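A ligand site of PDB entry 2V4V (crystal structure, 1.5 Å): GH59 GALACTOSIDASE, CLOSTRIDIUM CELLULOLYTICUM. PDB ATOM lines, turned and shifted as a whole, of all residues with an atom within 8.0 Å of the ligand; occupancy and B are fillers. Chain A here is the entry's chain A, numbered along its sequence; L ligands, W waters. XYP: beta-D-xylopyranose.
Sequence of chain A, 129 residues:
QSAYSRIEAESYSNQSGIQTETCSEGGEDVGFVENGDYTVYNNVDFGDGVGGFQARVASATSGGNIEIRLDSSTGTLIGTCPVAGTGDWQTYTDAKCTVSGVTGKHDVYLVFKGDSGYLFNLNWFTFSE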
ATOM      1  N   GLN A  19      -2.239   2.560  23.716  1.00  0.00           N
ATOM      2  CA  GLN A  19      -2.766   2.479  22.344  1.00  0.00           C
ATOM      3  C   GLN A  19      -2.392   1.135  21.761  1.00  0.00           C
ATOM      4  O   GLN A  19      -1.281   0.655  22.071  1.00  0.00           O
ATOM      5  CB  GLN A  19      -2.195   3.577  21.452  1.00  0.00           C
ATOM      6  CG  GLN A  19      -2.322   4.942  22.054  1.00  0.00           C
ATOM      7  CD  GLN A  19      -1.534   5.976  21.273  1.00  0.00           C
ATOM      8  OE1 GLN A  19      -1.487   5.913  20.013  1.00  0.00           O
ATOM      9  NE2 GLN A  19      -0.910   6.933  21.995  1.00  0.00           N
ATOM     10  N   GLU A  21      -1.453  -1.350  18.578  1.00  0.00           N
ATOM     11  CA  GLU A  21      -0.657  -1.212  17.352  1.00  0.00           C
ATOM     12  C   GLU A  21      -0.331  -2.568  16.767  1.00  0.00           C
ATOM     13  O   GLU A  21      -0.528  -3.618  17.425  1.00  0.00           O
ATOM     14  CB  GLU A  21       0.619  -0.422  17.601  1.00  0.00           C
ATOM     15  CG  GLU A  21       1.473  -1.108  18.676  1.00  0.00           C
ATOM     16  CD  GLU A  21       2.806  -0.424  18.943  1.00  0.00           C
ATOM     17  OE1 GLU A  21       3.199   0.545  18.220  1.00  0.00           O
ATOM     18  OE2 GLU A  21       3.473  -0.909  19.890  1.00  0.00           O
ATOM     19  N   THR A  22       0.221  -2.557  15.548  1.00  0.00           N
ATOM     20  CA  THR A  22       0.544  -3.805  14.830  1.00  0.00           C
ATOM     21  C   THR A  22       1.704  -4.478  15.554  1.00  0.00           C
ATOM     22  O   THR A  22       2.712  -3.838  15.819  1.00  0.00           O
ATOM     23  CB  THR A  22       1.025  -3.497  13.401  1.00  0.00           C
ATOM     24  OG1 THR A  22       0.046  -2.680  12.750  1.00  0.00           O
ATOM     25  CG2 THR A  22       1.223  -4.780  12.591  1.00  0.00           C
ATOM     26  N   ASP A  29      -0.277  -5.454  19.621  1.00  0.00           N
ATOM     27  CA  ASP A  29       0.184  -5.292  20.995  1.00  0.00           C
ATOM     28  C   ASP A  29      -0.388  -4.024  21.609  1.00  0.00           C
ATOM     29  O   ASP A  29      -0.710  -3.046  20.902  1.00  0.00           O
ATOM     30  CB  ASP A  29       1.733  -5.289  21.100  1.00  0.00           C
ATOM     31  CG  ASP A  29       2.362  -4.137  20.343  1.00  0.00           C
ATOM     32  OD1 ASP A  29       2.682  -4.329  19.127  1.00  0.00           O
ATOM     33  OD2 ASP A  29       2.514  -3.020  20.974  1.00  0.00           O
ATOM     34  N   VAL A  30      -0.484  -4.049  22.946  1.00  0.00           N
ATOM     35  CA  VAL A  30      -0.751  -2.846  23.695  1.00  0.00           C
ATOM     36  C   VAL A  30       0.610  -2.186  23.882  1.00  0.00           C
ATOM     37  O   VAL A  30       1.541  -2.779  24.485  1.00  0.00           O
ATOM     38  CB  VAL A  30      -1.387  -3.178  25.059  1.00  0.00           C
ATOM     39  CG1 VAL A  30      -1.248  -2.056  26.010  1.00  0.00           C
ATOM     40  CG2 VAL A  30      -2.867  -3.518  24.828  1.00  0.00           C
ATOM     41  N   GLY A  31       0.718  -0.988  23.318  1.00  0.00           N
ATOM     42  CA  GLY A  31       1.945  -0.202  23.449  1.00  0.00           C
ATOM     43  C   GLY A  31       1.681   1.204  24.015  1.00  0.00           C
ATOM     44  O   GLY A  31       0.609   1.498  24.522  1.00  0.00           O
ATOM     45  N   PHE A  32       2.702   2.046  23.878  1.00  0.00           N
ATOM     46  CA  PHE A  32       2.675   3.394  24.462  1.00  0.00           C
ATOM     47  C   PHE A  32       2.355   3.336  25.954  1.00  0.00           C
ATOM     48  O   PHE A  32       1.514   4.081  26.451  1.00  0.00           O
ATOM     49  CB  PHE A  32       1.694   4.269  23.687  1.00  0.00           C
ATOM     50  CG  PHE A  32       1.956   4.222  22.177  1.00  0.00           C
ATOM     51  CD1 PHE A  32       2.734   5.223  21.531  1.00  0.00           C
ATOM     52  CD2 PHE A  32       1.470   3.192  21.406  1.00  0.00           C
ATOM     53  CE1 PHE A  32       3.004   5.165  20.186  1.00  0.00           C
ATOM     54  CE2 PHE A  32       1.741   3.160  20.045  1.00  0.00           C
ATOM     55  CZ  PHE A  32       2.493   4.152  19.449  1.00  0.00           C
ATOM     56  N   VAL A  33       3.084   2.434  26.650  1.00  0.00           N
ATOM     57  CA  VAL A  33       2.842   2.176  28.085  1.00  0.00           C
ATOM     58  C   VAL A  33       3.805   3.010  28.900  1.00  0.00           C
ATOM     59  O   VAL A  33       5.043   2.872  28.778  1.00  0.00           O
ATOM     60  CB  VAL A  33       3.100   0.701  28.367  1.00  0.00           C
ATOM     61  CG1 VAL A  33       3.039   0.440  29.864  1.00  0.00           C
ATOM     62  CG2 VAL A  33       2.103  -0.180  27.583  1.00  0.00           C
ATOM     63  N   GLU A  34       3.214   3.860  29.749  1.00  0.00           N
ATOM     64  CA  GLU A  34       3.985   4.644  30.699  1.00  0.00           C
ATOM     65  C   GLU A  34       3.503   4.343  32.120  1.00  0.00           C
ATOM     66  O   GLU A  34       2.398   3.770  32.338  1.00  0.00           O
ATOM     67  CB  GLU A  34       3.852   6.144  30.434  1.00  0.00           C
ATOM     68  CG  GLU A  34       4.468   6.521  29.100  1.00  0.00           C
ATOM     69  CD  GLU A  34       4.428   8.020  28.872  1.00  0.00           C
ATOM     70  OE1 GLU A  34       5.260   8.749  29.491  1.00  0.00           O
ATOM     71  OE2 GLU A  34       3.589   8.480  28.066  1.00  0.00           O
ATOM     72  N   ALA A  58       7.577  -7.108  24.918  1.00  0.00           N
ATOM     73  CA  ALA A  58       8.767  -6.586  24.207  1.00  0.00           C
ATOM     74  C   ALA A  58       9.139  -5.234  24.839  1.00  0.00           C
ATOM     75  O   ALA A  58       8.263  -4.529  25.359  1.00  0.00           O
ATOM     76  CB  ALA A  58       8.459  -6.363  22.734  1.00  0.00           C
ATOM     77  N   SER A  59      10.435  -4.878  24.801  1.00  0.00           N
ATOM     78  CA  SER A  59      10.751  -3.533  25.272  1.00  0.00           C
ATOM     79  C   SER A  59      12.095  -3.075  24.736  1.00  0.00           C
ATOM     80  O   SER A  59      13.101  -3.831  24.868  1.00  0.00           O
ATOM     81  CB  SER A  59      10.866  -3.494  26.809  1.00  0.00           C
ATOM     82  OG  SER A  59      11.382  -2.250  27.239  1.00  0.00           O
ATOM     83  N   ALA A  60      12.144  -1.853  24.203  1.00  0.00           N
ATOM     84  CA  ALA A  60      13.422  -1.261  23.798  1.00  0.00           C
ATOM     85  C   ALA A  60      14.098  -0.494  24.911  1.00  0.00           C
ATOM     86  O   ALA A  60      15.152   0.151  24.712  1.00  0.00           O
ATOM     87  CB  ALA A  60      13.258  -0.351  22.597  1.00  0.00           C
ATOM     88  N   THR A  61      13.498  -0.550  26.098  1.00  0.00           N
ATOM     89  CA  THR A  61      14.038   0.191  27.222  1.00  0.00           C
ATOM     90  C   THR A  61      14.438  -0.839  28.290  1.00  0.00           C
ATOM     91  O   THR A  61      15.074  -1.854  27.963  1.00  0.00           O
ATOM     92  CB  THR A  61      12.996   1.218  27.748  1.00  0.00           C
ATOM     93  OG1 THR A  61      11.798   0.497  28.079  1.00  0.00           O
ATOM     94  CG2 THR A  61      12.695   2.325  26.653  1.00  0.00           C
ATOM     95  N   ASP A  88      14.283  -4.365  21.547  1.00  0.00           N
ATOM     96  CA  ASP A  88      13.501  -3.846  20.432  1.00  0.00           C
ATOM     97  C   ASP A  88      12.038  -3.853  20.813  1.00  0.00           C
ATOM     98  O   ASP A  88      11.601  -4.782  21.483  1.00  0.00           O
ATOM     99  CB  ASP A  88      13.715  -4.731  19.205  1.00  0.00           C
ATOM    100  CG  ASP A  88      13.158  -4.099  17.938  1.00  0.00           C
ATOM    101  OD1 ASP A  88      13.928  -3.320  17.310  1.00  0.00           O
ATOM    102  OD2 ASP A  88      12.000  -4.374  17.579  1.00  0.00           O
ATOM    103  N   TRP A  89      11.272  -2.840  20.358  1.00  0.00           N
ATOM    104  CA  TRP A  89       9.850  -2.805  20.674  1.00  0.00           C
ATOM    105  C   TRP A  89       9.025  -3.946  20.102  1.00  0.00           C
ATOM    106  O   TRP A  89       7.881  -4.143  20.517  1.00  0.00           O
ATOM    107  CB  TRP A  89       9.204  -1.489  20.176  1.00  0.00           C
ATOM    108  CG  TRP A  89       9.657  -0.288  20.970  1.00  0.00           C
ATOM    109  CD1 TRP A  89      10.331   0.809  20.495  1.00  0.00           C
ATOM    110  CD2 TRP A  89       9.486  -0.083  22.377  1.00  0.00           C
ATOM    111  NE1 TRP A  89      10.598   1.696  21.537  1.00  0.00           N
ATOM    112  CE2 TRP A  89      10.097   1.171  22.705  1.00  0.00           C
ATOM    113  CE3 TRP A  89       8.905  -0.825  23.416  1.00  0.00           C
ATOM    114  CZ2 TRP A  89      10.094   1.697  24.009  1.00  0.00           C
ATOM    115  CZ3 TRP A  89       8.887  -0.281  24.725  1.00  0.00           C
ATOM    116  CH2 TRP A  89       9.507   0.945  25.012  1.00  0.00           C
ATOM    117  N   GLN A  90       9.593  -4.653  19.128  1.00  0.00           N
ATOM    118  CA  GLN A  90       8.857  -5.751  18.472  1.00  0.00           C
ATOM    119  C   GLN A  90       9.603  -7.093  18.470  1.00  0.00           C
ATOM    120  O   GLN A  90       9.327  -7.959  17.637  1.00  0.00           O
ATOM    121  CB  GLN A  90       8.435  -5.329  17.049  1.00  0.00           C
ATOM    122  CG  GLN A  90       7.474  -4.135  17.007  1.00  0.00           C
ATOM    123  CD  GLN A  90       6.086  -4.467  17.596  1.00  0.00           C
ATOM    124  OE1 GLN A  90       5.703  -5.654  17.700  1.00  0.00           O
ATOM    125  NE2 GLN A  90       5.330  -3.435  17.973  1.00  0.00           N
ATOM    126  N   TYR A  92       9.817 -10.079  21.099  1.00  0.00           N
ATOM    127  CA  TYR A  92       9.078 -10.486  22.317  1.00  0.00           C
ATOM    128  C   TYR A  92       9.765 -11.630  23.046  1.00  0.00           C
ATOM    129  O   TYR A  92      10.517 -12.409  22.464  1.00  0.00           O
ATOM    130  CB  TYR A  92       7.620 -10.840  22.015  1.00  0.00           C
ATOM    131  CG  TYR A  92       6.837  -9.648  21.509  1.00  0.00           C
ATOM    132  CD1 TYR A  92       5.925  -8.993  22.330  1.00  0.00           C
ATOM    133  CD2 TYR A  92       7.072  -9.123  20.207  1.00  0.00           C
ATOM    134  CE1 TYR A  92       5.214  -7.888  21.896  1.00  0.00           C
ATOM    135  CE2 TYR A  92       6.362  -8.008  19.742  1.00  0.00           C
ATOM    136  CZ  TYR A  92       5.455  -7.363  20.607  1.00  0.00           C
ATOM    137  OH  TYR A  92       4.736  -6.236  20.221  1.00  0.00           O
ATOM    138  N   GLY A 117       9.574   7.176  30.928  1.00  0.00           N
ATOM    139  CA  GLY A 117       9.601   6.750  29.535  1.00  0.00           C
ATOM    140  C   GLY A 117       8.678   5.575  29.288  1.00  0.00           C
ATOM    141  O   GLY A 117       7.882   5.203  30.153  1.00  0.00           O
ATOM    142  N   TYR A 118       8.763   4.979  28.098  1.00  0.00           N
ATOM    143  CA  TYR A 118       7.910   3.853  27.775  1.00  0.00           C
ATOM    144  C   TYR A 118       8.488   2.579  28.377  1.00  0.00           C
ATOM    145  O   TYR A 118       9.725   2.412  28.433  1.00  0.00           O
ATOM    146  CB  TYR A 118       7.853   3.711  26.285  1.00  0.00           C
ATOM    147  CG  TYR A 118       7.191   4.853  25.592  1.00  0.00           C
ATOM    148  CD1 TYR A 118       5.826   5.120  25.755  1.00  0.00           C
ATOM    149  CD2 TYR A 118       7.909   5.640  24.694  1.00  0.00           C
ATOM    150  CE1 TYR A 118       5.210   6.172  25.068  1.00  0.00           C
ATOM    151  CE2 TYR A 118       7.297   6.684  23.998  1.00  0.00           C
ATOM    152  CZ  TYR A 118       5.940   6.921  24.174  1.00  0.00           C
ATOM    153  OH  TYR A 118       5.333   7.954  23.468  1.00  0.00           O
ATOM    154  N   LEU A 119       7.588   1.705  28.832  1.00  0.00           N
ATOM    155  CA  LEU A 119       8.036   0.555  29.608  1.00  0.00           C
ATOM    156  C   LEU A 119       8.162  -0.744  28.767  1.00  0.00           C
ATOM    157  O   LEU A 119       9.257  -1.379  28.735  1.00  0.00           O
ATOM    158  CB  LEU A 119       7.085   0.315  30.794  1.00  0.00           C
ATOM    159  CG  LEU A 119       6.877   1.539  31.702  1.00  0.00           C
ATOM    160  CD1 LEU A 119       5.983   1.108  32.801  1.00  0.00           C
ATOM    161  CD2 LEU A 119       8.144   2.123  32.282  1.00  0.00           C
ATOM    162  N   PHE A 120       7.059  -1.179  28.159  1.00  0.00           N
ATOM    163  CA  PHE A 120       7.097  -2.423  27.368  1.00  0.00           C
ATOM    164  C   PHE A 120       5.814  -2.464  26.548  1.00  0.00           C
ATOM    165  O   PHE A 120       4.893  -1.610  26.776  1.00  0.00           O
ATOM    166  CB  PHE A 120       7.147  -3.686  28.282  1.00  0.00           C
ATOM    167  CG  PHE A 120       6.226  -3.582  29.529  1.00  0.00           C
ATOM    168  CD1 PHE A 120       4.839  -3.751  29.439  1.00  0.00           C
ATOM    169  CD2 PHE A 120       6.776  -3.230  30.776  1.00  0.00           C
ATOM    170  CE1 PHE A 120       4.037  -3.588  30.611  1.00  0.00           C
ATOM    171  CE2 PHE A 120       5.996  -3.075  31.925  1.00  0.00           C
ATOM    172  CZ  PHE A 120       4.638  -3.264  31.838  1.00  0.00           C
ATOM    173  N   ASN A 121       5.799  -3.357  25.554  1.00  0.00           N
ATOM    174  CA  ASN A 121       4.597  -3.661  24.754  1.00  0.00           C
ATOM    175  C   ASN A 121       4.094  -5.047  25.213  1.00  0.00           C
ATOM    176  O   ASN A 121       4.914  -5.936  25.526  1.00  0.00           O
ATOM    177  CB  ASN A 121       4.943  -3.741  23.255  1.00  0.00           C
ATOM    178  CG  ASN A 121       5.320  -2.410  22.660  1.00  0.00           C
ATOM    179  OD1 ASN A 121       5.994  -2.335  21.587  1.00  0.00           O
ATOM    180  ND2 ASN A 121       4.947  -1.357  23.358  1.00  0.00           N
ATOM    181  N   LEU A 122       2.759  -5.231  25.208  1.00  0.00           N
ATOM    182  CA  LEU A 122       2.171  -6.498  25.706  1.00  0.00           C
ATOM    183  C   LEU A 122       1.359  -7.083  24.576  1.00  0.00           C
ATOM    184  O   LEU A 122       0.444  -6.436  24.087  1.00  0.00           O
ATOM    185  CB  LEU A 122       1.283  -6.226  26.950  1.00  0.00           C
ATOM    186  CG  LEU A 122       0.473  -7.391  27.522  1.00  0.00           C
ATOM    187  CD1 LEU A 122       1.412  -8.473  28.144  1.00  0.00           C
ATOM    188  CD2 LEU A 122      -0.425  -6.808  28.615  1.00  0.00           C
HETATM  189  O1  XYP L   1       7.300   4.549  19.056  1.00  0.00           O
HETATM  190  C1  XYP L   1       6.539   3.854  20.031  1.00  0.00           C
HETATM  191  C2  XYP L   1       6.447   2.413  19.545  1.00  0.00           C
HETATM  192  C3  XYP L   1       5.684   1.577  20.556  1.00  0.00           C
HETATM  193  C4  XYP L   1       6.223   1.805  21.964  1.00  0.00           C
HETATM  194  C5  XYP L   1       6.352   3.309  22.256  1.00  0.00           C
HETATM  195  O2  XYP L   1       5.741   2.304  18.326  1.00  0.00           O
HETATM  196  O3  XYP L   1       5.746   0.200  20.211  1.00  0.00           O
HETATM  197  O4  XYP L   1       5.372   1.239  22.934  1.00  0.00           O
HETATM  198  O5  XYP L   1       7.139   3.916  21.266  1.00  0.00           O
HETATM  199  O   HOH W   1      10.299   3.977  18.489  1.00  0.00           O
HETATM  200  O   HOH W   2       6.614  -0.670  17.683  1.00  0.00           O
HETATM  201  O   HOH W   3       9.760   4.953  21.697  1.00  0.00           O
HETATM  202  O   HOH W   4       5.411   0.938  25.656  1.00  0.00           O
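O3 of the ligand sits at hydrogen-bond distance from OE2 of Glu 21, 2.5 Å away.
The side-chain amide nitrogen (ND2) of Asn 121 is in hydrogen-bond range of an oxygen (O4) of the ligand.
O4 of the ligand lies within hydrogen-bond range of N of Phe 32, 2.9 Å away.
The side-chain carboxylate (OE2) of Glu 21 sits close to the side-chain amide oxygen (OD1) of Asn 121.
O of Glu 21 sits at hydrogen-bond distance from N of Asp 29 (2.9 Å).
The side-chain amide oxygen (OD1) of Asn 121 lies close to the backbone carbonyl oxygen (O) of Trp 89, at 2.8 Å.
N of Asn 121 lies within hydrogen-bond range of O of Ala 58, at 2.7 Å.
The backbone carbonyl oxygen of Tyr 118 lies within hydrogen-bond range of the side-chain hydroxyl of Thr 61, 2.8 Å away.
The backbone NH (N) of Gly 31 is in hydrogen-bond range of the backbone carbonyl oxygen (O) of Gln 19, 2.9 Å away.
Merely in contact with the ligand: Gly 31, Trp 89 and Tyr 118.
Six residues have an atom within 4 Å of the ligand: Glu 21, Gly 31, Phe 32, Trp 89, Tyr 118 and Asn 121.
The nearest printed residue that does not touch the ligand is Gln 90 (4.3 Å).
Water W2 bridges an oxygen (O3) of the ligand (2.8 Å) and the side-chain amide nitrogen of Gln 90 (3.1 Å).
Water W3 lies within hydrogen-bond range of an oxygen (O5) of the ligand (2.9 Å) and the indole nitrogen of Trp 89 (3.4 Å).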
